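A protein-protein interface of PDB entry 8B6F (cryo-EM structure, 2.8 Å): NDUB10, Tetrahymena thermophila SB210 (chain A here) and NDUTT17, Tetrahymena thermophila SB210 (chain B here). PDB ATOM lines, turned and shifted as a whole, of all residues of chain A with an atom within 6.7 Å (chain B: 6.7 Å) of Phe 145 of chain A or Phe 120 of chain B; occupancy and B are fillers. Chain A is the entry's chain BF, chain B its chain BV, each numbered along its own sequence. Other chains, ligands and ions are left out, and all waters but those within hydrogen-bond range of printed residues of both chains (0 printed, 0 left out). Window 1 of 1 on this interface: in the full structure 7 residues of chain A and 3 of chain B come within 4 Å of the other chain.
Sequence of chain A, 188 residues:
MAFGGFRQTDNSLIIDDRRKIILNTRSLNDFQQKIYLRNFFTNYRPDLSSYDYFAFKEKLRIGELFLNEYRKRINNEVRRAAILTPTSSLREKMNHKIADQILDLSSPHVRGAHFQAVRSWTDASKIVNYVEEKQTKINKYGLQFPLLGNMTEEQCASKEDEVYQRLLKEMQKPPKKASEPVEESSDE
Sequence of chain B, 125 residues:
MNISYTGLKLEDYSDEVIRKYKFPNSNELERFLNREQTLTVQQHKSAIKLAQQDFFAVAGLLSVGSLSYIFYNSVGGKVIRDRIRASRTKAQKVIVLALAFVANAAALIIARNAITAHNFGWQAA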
ATOM      1  N   ILE A 138     -20.631   3.563  37.892  1.00  0.00           N
ATOM      2  CA  ILE A 138     -19.783   3.130  36.786  1.00  0.00           C
ATOM      3  C   ILE A 138     -19.466   4.299  35.863  1.00  0.00           C
ATOM      4  O   ILE A 138     -18.311   4.510  35.478  1.00  0.00           O
ATOM      5  CB  ILE A 138     -20.457   1.969  36.029  1.00  0.00           C
ATOM      6  CG1 ILE A 138     -20.236   0.658  36.782  1.00  0.00           C
ATOM      7  CG2 ILE A 138     -19.951   1.870  34.590  1.00  0.00           C
ATOM      8  CD1 ILE A 138     -21.079  -0.479  36.278  1.00  0.00           C
ATOM      9  N   GLY A 142     -16.412   6.054  33.830  1.00  0.00           N
ATOM     10  CA  GLY A 142     -16.492   5.680  32.430  1.00  0.00           C
ATOM     11  C   GLY A 142     -16.028   4.269  32.146  1.00  0.00           C
ATOM     12  O   GLY A 142     -15.289   4.045  31.181  1.00  0.00           O
ATOM     13  N   LEU A 143     -16.449   3.307  32.962  1.00  0.00           N
ATOM     14  CA  LEU A 143     -16.091   1.911  32.775  1.00  0.00           C
ATOM     15  C   LEU A 143     -17.015   1.193  31.803  1.00  0.00           C
ATOM     16  O   LEU A 143     -16.865  -0.017  31.611  1.00  0.00           O
ATOM     17  CB  LEU A 143     -16.108   1.171  34.118  1.00  0.00           C
ATOM     18  CG  LEU A 143     -15.117   1.616  35.191  1.00  0.00           C
ATOM     19  CD1 LEU A 143     -15.702   1.401  36.570  1.00  0.00           C
ATOM     20  CD2 LEU A 143     -13.815   0.853  35.039  1.00  0.00           C
ATOM     21  N   GLN A 144     -17.965   1.900  31.191  1.00  0.00           N
ATOM     22  CA  GLN A 144     -19.007   1.268  30.395  1.00  0.00           C
ATOM     23  C   GLN A 144     -18.831   1.488  28.896  1.00  0.00           C
ATOM     24  O   GLN A 144     -19.784   1.302  28.136  1.00  0.00           O
ATOM     25  CB  GLN A 144     -20.380   1.772  30.848  1.00  0.00           C
ATOM     26  CG  GLN A 144     -20.850   3.081  30.204  1.00  0.00           C
ATOM     27  CD  GLN A 144     -19.826   4.196  30.292  1.00  0.00           C
ATOM     28  OE1 GLN A 144     -18.855   4.108  31.038  1.00  0.00           O
ATOM     29  NE2 GLN A 144     -20.045   5.258  29.528  1.00  0.00           N
ATOM     30  N   PHE A 145     -17.633   1.868  28.444  1.00  0.00           N
ATOM     31  CA  PHE A 145     -17.464   2.165  27.022  1.00  0.00           C
ATOM     32  C   PHE A 145     -17.675   0.923  26.172  1.00  0.00           C
ATOM     33  O   PHE A 145     -18.624   0.893  25.369  1.00  0.00           O
ATOM     34  CB  PHE A 145     -16.091   2.787  26.763  1.00  0.00           C
ATOM     35  CG  PHE A 145     -15.595   2.573  25.358  1.00  0.00           C
ATOM     36  CD1 PHE A 145     -16.369   2.956  24.275  1.00  0.00           C
ATOM     37  CD2 PHE A 145     -14.355   2.004  25.120  1.00  0.00           C
ATOM     38  CE1 PHE A 145     -15.922   2.765  22.984  1.00  0.00           C
ATOM     39  CE2 PHE A 145     -13.903   1.809  23.829  1.00  0.00           C
ATOM     40  CZ  PHE A 145     -14.688   2.189  22.761  1.00  0.00           C
ATOM     41  N   PRO A 146     -16.846  -0.118  26.277  1.00  0.00           N
ATOM     42  CA  PRO A 146     -17.069  -1.296  25.430  1.00  0.00           C
ATOM     43  C   PRO A 146     -18.256  -2.120  25.888  1.00  0.00           C
ATOM     44  O   PRO A 146     -19.053  -2.568  25.056  1.00  0.00           O
ATOM     45  CB  PRO A 146     -15.747  -2.061  25.556  1.00  0.00           C
ATOM     46  CG  PRO A 146     -15.281  -1.736  26.926  1.00  0.00           C
ATOM     47  CD  PRO A 146     -15.743  -0.330  27.230  1.00  0.00           C
ATOM     48  N   LEU A 147     -18.397  -2.323  27.193  1.00  0.00           N
ATOM     49  CA  LEU A 147     -19.504  -3.074  27.763  1.00  0.00           C
ATOM     50  C   LEU A 147     -20.520  -2.108  28.352  1.00  0.00           C
ATOM     51  O   LEU A 147     -20.153  -1.087  28.938  1.00  0.00           O
ATOM     52  CB  LEU A 147     -19.012  -4.029  28.853  1.00  0.00           C
ATOM     53  CG  LEU A 147     -18.264  -5.297  28.431  1.00  0.00           C
ATOM     54  CD1 LEU A 147     -17.044  -4.991  27.584  1.00  0.00           C
ATOM     55  CD2 LEU A 147     -17.859  -6.089  29.661  1.00  0.00           C
ATOM     56  N   LEU A 148     -21.800  -2.437  28.197  1.00  0.00           N
ATOM     57  CA  LEU A 148     -22.885  -1.622  28.740  1.00  0.00           C
ATOM     58  C   LEU A 148     -22.825  -0.191  28.213  1.00  0.00           C
ATOM     59  O   LEU A 148     -23.052   0.769  28.951  1.00  0.00           O
ATOM     60  CB  LEU A 148     -22.866  -1.628  30.271  1.00  0.00           C
ATOM     61  CG  LEU A 148     -22.969  -2.994  30.950  1.00  0.00           C
ATOM     62  CD1 LEU A 148     -22.877  -2.835  32.452  1.00  0.00           C
ATOM     63  CD2 LEU A 148     -24.258  -3.705  30.564  1.00  0.00           C
ATOM     64  N   GLY A 149     -22.521  -0.040  26.927  1.00  0.00           N
ATOM     65  CA  GLY A 149     -22.492   1.280  26.330  1.00  0.00           C
ATOM     66  C   GLY A 149     -21.811   1.344  24.978  1.00  0.00           C
ATOM     67  O   GLY A 149     -20.973   0.501  24.653  1.00  0.00           O
ATOM     68  N   ASN A 150     -22.177   2.345  24.179  1.00  0.00           N
ATOM     69  CA  ASN A 150     -21.561   2.591  22.885  1.00  0.00           C
ATOM     70  C   ASN A 150     -21.292   4.082  22.747  1.00  0.00           C
ATOM     71  O   ASN A 150     -22.148   4.906  23.080  1.00  0.00           O
ATOM     72  CB  ASN A 150     -22.456   2.114  21.734  1.00  0.00           C
ATOM     73  CG  ASN A 150     -22.650   0.614  21.728  1.00  0.00           C
ATOM     74  OD1 ASN A 150     -21.716  -0.145  21.984  1.00  0.00           O
ATOM     75  ND2 ASN A 150     -23.868   0.176  21.440  1.00  0.00           N
ATOM     76  N   MET A 151     -20.103   4.423  22.258  1.00  0.00           N
ATOM     77  CA  MET A 151     -19.715   5.817  22.108  1.00  0.00           C
ATOM     78  C   MET A 151     -18.802   5.953  20.900  1.00  0.00           C
ATOM     79  O   MET A 151     -18.190   4.984  20.446  1.00  0.00           O
ATOM     80  CB  MET A 151     -19.009   6.342  23.363  1.00  0.00           C
ATOM     81  CG  MET A 151     -19.841   6.239  24.630  1.00  0.00           C
ATOM     82  SD  MET A 151     -19.128   7.149  26.014  1.00  0.00           S
ATOM     83  CE  MET A 151     -17.510   6.396  26.130  1.00  0.00           C
ATOM     84  N   THR A 152     -18.718   7.176  20.384  1.00  0.00           N
ATOM     85  CA  THR A 152     -17.843   7.483  19.266  1.00  0.00           C
ATOM     86  C   THR A 152     -16.446   7.827  19.778  1.00  0.00           C
ATOM     87  O   THR A 152     -16.193   7.879  20.983  1.00  0.00           O
ATOM     88  CB  THR A 152     -18.416   8.628  18.432  1.00  0.00           C
ATOM     89  OG1 THR A 152     -18.500   9.815  19.232  1.00  0.00           O
ATOM     90  CG2 THR A 152     -19.797   8.273  17.912  1.00  0.00           C
ATOM     91  N   GLU A 153     -15.523   8.072  18.848  1.00  0.00           N
ATOM     92  CA  GLU A 153     -14.149   8.372  19.237  1.00  0.00           C
ATOM     93  C   GLU A 153     -14.062   9.687  19.999  1.00  0.00           C
ATOM     94  O   GLU A 153     -13.372   9.773  21.020  1.00  0.00           O
ATOM     95  CB  GLU A 153     -13.245   8.413  18.007  1.00  0.00           C
ATOM     96  CG  GLU A 153     -13.049   7.074  17.317  1.00  0.00           C
ATOM     97  CD  GLU A 153     -14.243   6.651  16.487  1.00  0.00           C
ATOM     98  OE1 GLU A 153     -15.304   7.303  16.589  1.00  0.00           O
ATOM     99  OE2 GLU A 153     -14.120   5.671  15.725  1.00  0.00           O
ATOM    100  N   CYS A 156     -15.389   9.165  23.421  1.00  0.00           N
ATOM    101  CA  CYS A 156     -14.435   8.440  24.253  1.00  0.00           C
ATOM    102  C   CYS A 156     -13.323   9.359  24.741  1.00  0.00           C
ATOM    103  O   CYS A 156     -12.930   9.302  25.912  1.00  0.00           O
ATOM    104  CB  CYS A 156     -13.851   7.260  23.479  1.00  0.00           C
ATOM    105  SG  CYS A 156     -15.055   6.000  23.024  1.00  0.00           S
ATOM    106  N   ALA B 117     -16.350  -4.754  14.666  1.00  0.00           N
ATOM    107  CA  ALA B 117     -16.074  -3.333  14.475  1.00  0.00           C
ATOM    108  C   ALA B 117     -14.624  -3.037  14.852  1.00  0.00           C
ATOM    109  O   ALA B 117     -14.314  -2.461  15.897  1.00  0.00           O
ATOM    110  CB  ALA B 117     -17.053  -2.493  15.287  1.00  0.00           C
ATOM    111  N   HIS B 118     -13.722  -3.455  13.963  1.00  0.00           N
ATOM    112  CA  HIS B 118     -12.301  -3.213  14.173  1.00  0.00           C
ATOM    113  C   HIS B 118     -11.915  -1.772  13.869  1.00  0.00           C
ATOM    114  O   HIS B 118     -11.016  -1.226  14.518  1.00  0.00           O
ATOM    115  CB  HIS B 118     -11.473  -4.159  13.302  1.00  0.00           C
ATOM    116  CG  HIS B 118     -11.683  -5.608  13.614  1.00  0.00           C
ATOM    117  ND1 HIS B 118     -12.101  -6.052  14.849  1.00  0.00           N
ATOM    118  CD2 HIS B 118     -11.536  -6.713  12.847  1.00  0.00           C
ATOM    119  CE1 HIS B 118     -12.198  -7.369  14.832  1.00  0.00           C
ATOM    120  NE2 HIS B 118     -11.862  -7.796  13.629  1.00  0.00           N
ATOM    121  N   ASN B 119     -12.575  -1.143  12.896  1.00  0.00           N
ATOM    122  CA  ASN B 119     -12.215   0.205  12.457  1.00  0.00           C
ATOM    123  C   ASN B 119     -12.835   1.232  13.406  1.00  0.00           C
ATOM    124  O   ASN B 119     -13.723   2.012  13.054  1.00  0.00           O
ATOM    125  CB  ASN B 119     -12.660   0.429  11.021  1.00  0.00           C
ATOM    126  CG  ASN B 119     -12.036  -0.563  10.061  1.00  0.00           C
ATOM    127  OD1 ASN B 119     -10.924  -0.358   9.574  1.00  0.00           O
ATOM    128  ND2 ASN B 119     -12.751  -1.646   9.782  1.00  0.00           N
ATOM    129  N   PHE B 120     -12.342   1.215  14.639  1.00  0.00           N
ATOM    130  CA  PHE B 120     -12.718   2.177  15.665  1.00  0.00           C
ATOM    131  C   PHE B 120     -11.470   2.958  16.046  1.00  0.00           C
ATOM    132  O   PHE B 120     -10.420   2.364  16.301  1.00  0.00           O
ATOM    133  CB  PHE B 120     -13.320   1.472  16.881  1.00  0.00           C
ATOM    134  CG  PHE B 120     -14.110   2.376  17.780  1.00  0.00           C
ATOM    135  CD1 PHE B 120     -15.443   2.640  17.521  1.00  0.00           C
ATOM    136  CD2 PHE B 120     -13.525   2.946  18.895  1.00  0.00           C
ATOM    137  CE1 PHE B 120     -16.171   3.465  18.350  1.00  0.00           C
ATOM    138  CE2 PHE B 120     -14.247   3.771  19.725  1.00  0.00           C
ATOM    139  CZ  PHE B 120     -15.569   4.031  19.453  1.00  0.00           C
ATOM    140  N   GLY B 121     -11.582   4.284  16.081  1.00  0.00           N
ATOM    141  CA  GLY B 121     -10.398   5.114  16.227  1.00  0.00           C
ATOM    142  C   GLY B 121      -9.807   5.143  17.620  1.00  0.00           C
ATOM    143  O   GLY B 121      -8.732   5.725  17.800  1.00  0.00           O
ATOM    144  N   TRP B 122     -10.465   4.529  18.598  1.00  0.00           N
ATOM    145  CA  TRP B 122     -10.016   4.594  19.983  1.00  0.00           C
ATOM    146  C   TRP B 122      -8.922   3.585  20.305  1.00  0.00           C
ATOM    147  O   TRP B 122      -8.444   3.558  21.443  1.00  0.00           O
ATOM    148  CB  TRP B 122     -11.205   4.389  20.924  1.00  0.00           C
ATOM    149  CG  TRP B 122     -10.879   4.623  22.365  1.00  0.00           C
ATOM    150  CD1 TRP B 122     -10.739   3.677  23.336  1.00  0.00           C
ATOM    151  CD2 TRP B 122     -10.643   5.885  22.995  1.00  0.00           C
ATOM    152  NE1 TRP B 122     -10.434   4.274  24.536  1.00  0.00           N
ATOM    153  CE2 TRP B 122     -10.370   5.630  24.353  1.00  0.00           C
ATOM    154  CE3 TRP B 122     -10.640   7.207  22.543  1.00  0.00           C
ATOM    155  CZ2 TRP B 122     -10.095   6.645  25.262  1.00  0.00           C
ATOM    156  CZ3 TRP B 122     -10.368   8.215  23.449  1.00  0.00           C
ATOM    157  CH2 TRP B 122     -10.100   7.930  24.794  1.00  0.00           C
ATOM    158  N   GLN B 123      -8.510   2.758  19.345  1.00  0.00           N
ATOM    159  CA  GLN B 123      -7.442   1.802  19.599  1.00  0.00           C
ATOM    160  C   GLN B 123      -6.190   2.545  20.043  1.00  0.00           C
ATOM    161  O   GLN B 123      -5.596   3.292  19.262  1.00  0.00           O
ATOM    162  CB  GLN B 123      -7.145   0.965  18.352  1.00  0.00           C
ATOM    163  CG  GLN B 123      -8.364   0.335  17.699  1.00  0.00           C
ATOM    164  CD  GLN B 123      -9.173  -0.521  18.648  1.00  0.00           C
ATOM    165  OE1 GLN B 123      -8.691  -0.924  19.705  1.00  0.00           O
ATOM    166  NE2 GLN B 123     -10.415  -0.803  18.274  1.00  0.00           N
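O of Thr 152 of chain A sits at hydrogen-bond distance from SG of Cys 156 of chain A (3.0 Å).
Among the printed residues, merely in contact across the chains: Met 151 of chain A with Phe 120 of chain B (3.0 Å), Cys 156 of chain A with Trp 122 of chain B (3.3 Å), Phe 145 of chain A with Phe 120 of chain B (3.5 Å), Phe 145 of chain A with Trp 122 of chain B (3.7 Å), Glu 153 of chain A with Phe 120 of chain B (3.8 Å), Glu 153 of chain A with Trp 122 of chain B (3.8 Å) and Thr 152 of chain A with Phe 120 of chain B (3.9 Å).
Of the 14 printed residues of chain A, 5 touch a printed residue of chain B.
Hydrophobic or aromatic side chains of chain A within 4 Å of the printed part of chain B: Phe 145.
Among the printed residues, 8 pairs touch across the chains.
N of Gly 121 of chain B is in hydrogen-bond range of OE2 of Glu 153 of chain A.
Gln 144 of chain A touches none of the printed residues of chain B.
Phe 145 of chain A touches two residues of chain B.
Printed residues of chain B within 4 Å of Met 151 of chain A: Phe 120.
Printed residues of chain B within 4 Å of Glu 153 of chain A: Phe 120 (3.8 Å), Gly 121 (2.9 Å) and Trp 122 (3.8 Å).
Printed residues of chain B within 4 Å of Cys 156 of chain A: Trp 122.
Ala 117 of chain B touches none of the printed residues of chain A.
Phe 120 of chain B touches four residues of chain A.
The nearest printed residue of chain B that does not touch Phe 145 of chain A is Gln 123 of chain B (6.9 Å).
The nearest residue of chain A that does not touch Phe 120 of chain B is Cys 156 of chain A (4.1 Å).
The nearest printed residue of chain A that does not touch Trp 122 of chain B is Thr 152 of chain A (5.8 Å).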
